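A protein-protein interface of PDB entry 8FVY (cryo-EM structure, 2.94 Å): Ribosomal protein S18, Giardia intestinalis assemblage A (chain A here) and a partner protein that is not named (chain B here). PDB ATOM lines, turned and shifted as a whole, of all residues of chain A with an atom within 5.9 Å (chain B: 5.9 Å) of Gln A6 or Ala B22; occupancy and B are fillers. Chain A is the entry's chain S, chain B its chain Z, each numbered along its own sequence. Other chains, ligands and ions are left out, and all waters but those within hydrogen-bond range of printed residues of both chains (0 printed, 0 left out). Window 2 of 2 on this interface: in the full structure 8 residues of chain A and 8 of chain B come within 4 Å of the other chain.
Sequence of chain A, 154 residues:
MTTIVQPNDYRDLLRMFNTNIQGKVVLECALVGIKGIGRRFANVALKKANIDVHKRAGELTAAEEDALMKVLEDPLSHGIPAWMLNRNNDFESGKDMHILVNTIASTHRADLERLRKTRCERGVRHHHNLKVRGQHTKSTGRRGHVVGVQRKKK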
ATOM      1  N   ILE A   4      14.213   5.810  13.885  1.00  0.00           N
ATOM      2  CA  ILE A   4      13.983   4.827  12.841  1.00  0.00           C
ATOM      3  C   ILE A   4      15.286   4.401  12.205  1.00  0.00           C
ATOM      4  O   ILE A   4      15.527   3.215  11.967  1.00  0.00           O
ATOM      5  CB  ILE A   4      13.037   5.415  11.787  1.00  0.00           C
ATOM      6  CG1 ILE A   4      11.818   6.026  12.437  1.00  0.00           C
ATOM      7  CG2 ILE A   4      12.598   4.351  10.874  1.00  0.00           C
ATOM      8  CD1 ILE A   4      11.331   5.283  13.579  1.00  0.00           C
ATOM      9  N   VAL A   5      16.110   5.361  11.927  1.00  0.00           N
ATOM     10  CA  VAL A   5      17.295   5.183  11.116  1.00  0.00           C
ATOM     11  C   VAL A   5      18.504   5.072  12.022  1.00  0.00           C
ATOM     12  O   VAL A   5      18.590   5.736  13.058  1.00  0.00           O
ATOM     13  CB  VAL A   5      17.422   6.350  10.131  1.00  0.00           C
ATOM     14  CG1 VAL A   5      18.803   6.441   9.593  1.00  0.00           C
ATOM     15  CG2 VAL A   5      16.446   6.167   9.044  1.00  0.00           C
ATOM     16  N   GLN A   6      19.433   4.219  11.637  1.00  0.00           N
ATOM     17  CA  GLN A   6      20.632   4.063  12.426  1.00  0.00           C
ATOM     18  C   GLN A   6      21.388   5.383  12.472  1.00  0.00           C
ATOM     19  O   GLN A   6      21.629   5.999  11.428  1.00  0.00           O
ATOM     20  CB  GLN A   6      21.527   2.979  11.845  1.00  0.00           C
ATOM     21  CG  GLN A   6      21.253   1.612  12.386  1.00  0.00           C
ATOM     22  CD  GLN A   6      22.271   0.602  11.946  1.00  0.00           C
ATOM     23  OE1 GLN A   6      23.430   0.932  11.701  1.00  0.00           O
ATOM     24  NE2 GLN A   6      21.840  -0.640  11.817  1.00  0.00           N
ATOM     25  N   PRO A   7      21.779   5.846  13.648  1.00  0.00           N
ATOM     26  CA  PRO A   7      22.596   7.050  13.715  1.00  0.00           C
ATOM     27  C   PRO A   7      23.952   6.803  13.095  1.00  0.00           C
ATOM     28  O   PRO A   7      24.434   5.671  13.022  1.00  0.00           O
ATOM     29  CB  PRO A   7      22.709   7.319  15.216  1.00  0.00           C
ATOM     30  CG  PRO A   7      21.619   6.565  15.823  1.00  0.00           C
ATOM     31  CD  PRO A   7      21.417   5.375  14.990  1.00  0.00           C
ATOM     32  N   ASN A   8      24.579   7.894  12.669  1.00  0.00           N
ATOM     33  CA  ASN A   8      25.842   7.793  11.957  1.00  0.00           C
ATOM     34  C   ASN A   8      26.873   7.028  12.770  1.00  0.00           C
ATOM     35  O   ASN A   8      27.787   6.418  12.204  1.00  0.00           O
ATOM     36  CB  ASN A   8      26.347   9.189  11.642  1.00  0.00           C
ATOM     37  CG  ASN A   8      25.647   9.809  10.457  1.00  0.00           C
ATOM     38  OD1 ASN A   8      24.419   9.858  10.408  1.00  0.00           O
ATOM     39  ND2 ASN A   8      26.420  10.288   9.496  1.00  0.00           N
ATOM     40  N   ASP A   9      26.742   7.047  14.091  1.00  0.00           N
ATOM     41  CA  ASP A   9      27.688   6.403  14.989  1.00  0.00           C
ATOM     42  C   ASP A   9      27.192   5.073  15.522  1.00  0.00           C
ATOM     43  O   ASP A   9      27.817   4.511  16.424  1.00  0.00           O
ATOM     44  CB  ASP A   9      28.005   7.329  16.160  1.00  0.00           C
ATOM     45  CG  ASP A   9      26.850   7.449  17.137  1.00  0.00           C
ATOM     46  OD1 ASP A   9      26.510   6.442  17.794  1.00  0.00           O
ATOM     47  OD2 ASP A   9      26.290   8.558  17.259  1.00  0.00           O
ATOM     48  N   TYR A  10      26.080   4.567  15.002  1.00  0.00           N
ATOM     49  CA  TYR A  10      25.553   3.295  15.468  1.00  0.00           C
ATOM     50  C   TYR A  10      26.648   2.252  15.525  1.00  0.00           C
ATOM     51  O   TYR A  10      27.488   2.159  14.628  1.00  0.00           O
ATOM     52  CB  TYR A  10      24.438   2.834  14.551  1.00  0.00           C
ATOM     53  CG  TYR A  10      23.750   1.569  14.989  1.00  0.00           C
ATOM     54  CD1 TYR A  10      24.259   0.336  14.646  1.00  0.00           C
ATOM     55  CD2 TYR A  10      22.582   1.609  15.718  1.00  0.00           C
ATOM     56  CE1 TYR A  10      23.634  -0.814  15.029  1.00  0.00           C
ATOM     57  CE2 TYR A  10      21.949   0.466  16.100  1.00  0.00           C
ATOM     58  CZ  TYR A  10      22.477  -0.744  15.758  1.00  0.00           C
ATOM     59  OH  TYR A  10      21.838  -1.891  16.149  1.00  0.00           O
ATOM     60  N   ARG A  11      26.634   1.478  16.596  1.00  0.00           N
ATOM     61  CA  ARG A  11      27.681   0.520  16.896  1.00  0.00           C
ATOM     62  C   ARG A  11      27.032  -0.845  17.048  1.00  0.00           C
ATOM     63  O   ARG A  11      26.356  -1.114  18.043  1.00  0.00           O
ATOM     64  CB  ARG A  11      28.446   0.975  18.137  1.00  0.00           C
ATOM     65  CG  ARG A  11      29.014  -0.070  18.999  1.00  0.00           C
ATOM     66  CD  ARG A  11      29.937   0.530  20.086  1.00  0.00           C
ATOM     67  NE  ARG A  11      29.223   1.165  21.188  1.00  0.00           N
ATOM     68  CZ  ARG A  11      29.029   2.470  21.330  1.00  0.00           C
ATOM     69  NH1 ARG A  11      29.484   3.344  20.450  1.00  0.00           N
ATOM     70  NH2 ARG A  11      28.358   2.911  22.384  1.00  0.00           N
ATOM     71  N   ASP A  12      27.250  -1.703  16.052  1.00  0.00           N
ATOM     72  CA  ASP A  12      26.378  -2.849  15.820  1.00  0.00           C
ATOM     73  C   ASP A  12      26.465  -3.883  16.921  1.00  0.00           C
ATOM     74  O   ASP A  12      25.565  -4.716  17.064  1.00  0.00           O
ATOM     75  CB  ASP A  12      26.734  -3.503  14.492  1.00  0.00           C
ATOM     76  CG  ASP A  12      25.526  -3.733  13.612  1.00  0.00           C
ATOM     77  OD1 ASP A  12      24.548  -4.339  14.091  1.00  0.00           O
ATOM     78  OD2 ASP A  12      25.558  -3.309  12.439  1.00  0.00           O
ATOM     79  N   LEU B  20      16.348  -1.414  13.864  1.00  0.00           N
ATOM     80  CA  LEU B  20      16.597  -0.062  13.398  1.00  0.00           C
ATOM     81  C   LEU B  20      17.002  -0.111  11.938  1.00  0.00           C
ATOM     82  O   LEU B  20      17.836  -0.934  11.550  1.00  0.00           O
ATOM     83  CB  LEU B  20      17.684   0.589  14.229  1.00  0.00           C
ATOM     84  CG  LEU B  20      17.199   1.332  15.466  1.00  0.00           C
ATOM     85  CD1 LEU B  20      18.339   1.803  16.311  1.00  0.00           C
ATOM     86  CD2 LEU B  20      16.347   2.487  15.082  1.00  0.00           C
ATOM     87  N   PHE B  21      16.421   0.767  11.134  1.00  0.00           N
ATOM     88  CA  PHE B  21      16.707   0.753   9.714  1.00  0.00           C
ATOM     89  C   PHE B  21      18.060   1.392   9.459  1.00  0.00           C
ATOM     90  O   PHE B  21      18.344   2.491   9.935  1.00  0.00           O
ATOM     91  CB  PHE B  21      15.656   1.527   8.936  1.00  0.00           C
ATOM     92  CG  PHE B  21      14.725   0.670   8.184  1.00  0.00           C
ATOM     93  CD1 PHE B  21      15.181  -0.225   7.257  1.00  0.00           C
ATOM     94  CD2 PHE B  21      13.374   0.822   8.351  1.00  0.00           C
ATOM     95  CE1 PHE B  21      14.304  -1.002   6.566  1.00  0.00           C
ATOM     96  CE2 PHE B  21      12.494   0.066   7.659  1.00  0.00           C
ATOM     97  CZ  PHE B  21      12.952  -0.846   6.763  1.00  0.00           C
ATOM     98  N   ALA B  22      18.885   0.719   8.672  1.00  0.00           N
ATOM     99  CA  ALA B  22      20.180   1.266   8.294  1.00  0.00           C
ATOM    100  C   ALA B  22      19.999   2.224   7.122  1.00  0.00           C
ATOM    101  O   ALA B  22      20.178   1.883   5.952  1.00  0.00           O
ATOM    102  CB  ALA B  22      21.149   0.147   7.964  1.00  0.00           C
ATOM    103  N   ASP B  23      19.643   3.454   7.468  1.00  0.00           N
ATOM    104  CA  ASP B  23      19.648   4.625   6.579  1.00  0.00           C
ATOM    105  C   ASP B  23      18.809   4.339   5.335  1.00  0.00           C
ATOM    106  O   ASP B  23      17.625   4.004   5.468  1.00  0.00           O
ATOM    107  CB  ASP B  23      21.083   5.030   6.305  1.00  0.00           C
ATOM    108  CG  ASP B  23      21.916   3.904   5.718  1.00  0.00           C
ATOM    109  OD1 ASP B  23      21.935   3.750   4.481  1.00  0.00           O
ATOM    110  OD2 ASP B  23      22.549   3.170   6.500  1.00  0.00           O
ATOM    111  N   GLU B  24      19.366   4.473   4.134  1.00  0.00           N
ATOM    112  CA  GLU B  24      18.597   4.596   2.904  1.00  0.00           C
ATOM    113  C   GLU B  24      17.577   3.473   2.770  1.00  0.00           C
ATOM    114  O   GLU B  24      16.664   3.551   1.942  1.00  0.00           O
ATOM    115  CB  GLU B  24      19.523   4.562   1.692  1.00  0.00           C
ATOM    116  CG  GLU B  24      18.966   5.078   0.351  1.00  0.00           C
ATOM    117  CD  GLU B  24      18.125   6.347   0.416  1.00  0.00           C
ATOM    118  OE1 GLU B  24      17.673   6.798  -0.655  1.00  0.00           O
ATOM    119  OE2 GLU B  24      17.999   6.960   1.490  1.00  0.00           O
ATOM    120  N   ALA B  25      17.766   2.400   3.541  1.00  0.00           N
ATOM    121  CA  ALA B  25      16.865   1.260   3.486  1.00  0.00           C
ATOM    122  C   ALA B  25      15.418   1.666   3.719  1.00  0.00           C
ATOM    123  O   ALA B  25      14.514   1.128   3.074  1.00  0.00           O
ATOM    124  CB  ALA B  25      17.300   0.220   4.511  1.00  0.00           C
ATOM    125  N   ALA B  26      15.175   2.614   4.623  1.00  0.00           N
ATOM    126  CA  ALA B  26      13.801   2.984   4.935  1.00  0.00           C
ATOM    127  C   ALA B  26      13.030   3.339   3.674  1.00  0.00           C
ATOM    128  O   ALA B  26      11.976   2.757   3.390  1.00  0.00           O
ATOM    129  CB  ALA B  26      13.774   4.158   5.910  1.00  0.00           C
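Printed residues of chain A that touch a printed residue of chain B: Ile A4, Val A5, Gln A6 and Tyr A10. Of the 7 printed residues of chain B, 4 touch a printed residue of chain A. Hydrophobic or aromatic side chains of chain B that line the printed part of chain A: Leu B20, Phe B21 and Ala B22. Among the printed residues, no Asp or Glu carboxylate lies within 4 Å of a Lys or Arg side-chain nitrogen of the other chain.
Among the printed residues, pairs that only touch across the chains: Val A5 with Phe B21 (3.1 Å), Ile A4 with Leu B20 (3.3 Å), Val A5 with Asp B23 (3.6 Å), Tyr A10 with Leu B20 (3.9 Å) and Gln A6 with Ala B22 (3.99 Å).
The backbone carbonyl oxygen of Phe B21 sits at hydrogen-bond distance from the backbone NH of Gln A6 (2.7 Å). The backbone carbonyl oxygen (O) of Ile A4 sits at hydrogen-bond distance from the backbone NH (N) of Phe B21, 2.7 Å away.
Printed residues of chain B within 4 Å of Gln A6: Phe B21 (2.7 Å) and Ala B22 (3.99 Å). Of the printed residues of chain A, Asp B23 touches Val A5. Printed residues of chain A within 4 Å of Leu B20: Ile A4 and Tyr A10. Printed residues of chain B within 4 Å of Ile A4: Leu B20 (3.3 Å) and Phe B21 (2.7 Å). Printed residues of chain B within 4 Å of Tyr A10: Leu B20 (3.9 Å). Printed residues of chain B within 4 Å of Val A5: Phe B21 (3.1 Å) and Asp B23 (3.6 Å). The nearest printed residue of chain B that does not touch Gln A6 is Leu B20 (4.02 Å). The nearest printed residue of chain A that does not touch Ala B22 is Val A5 (5.0 Å). The nearest printed residue of chain A that does not touch Asp B23 is Gln A6 (4.2 Å).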
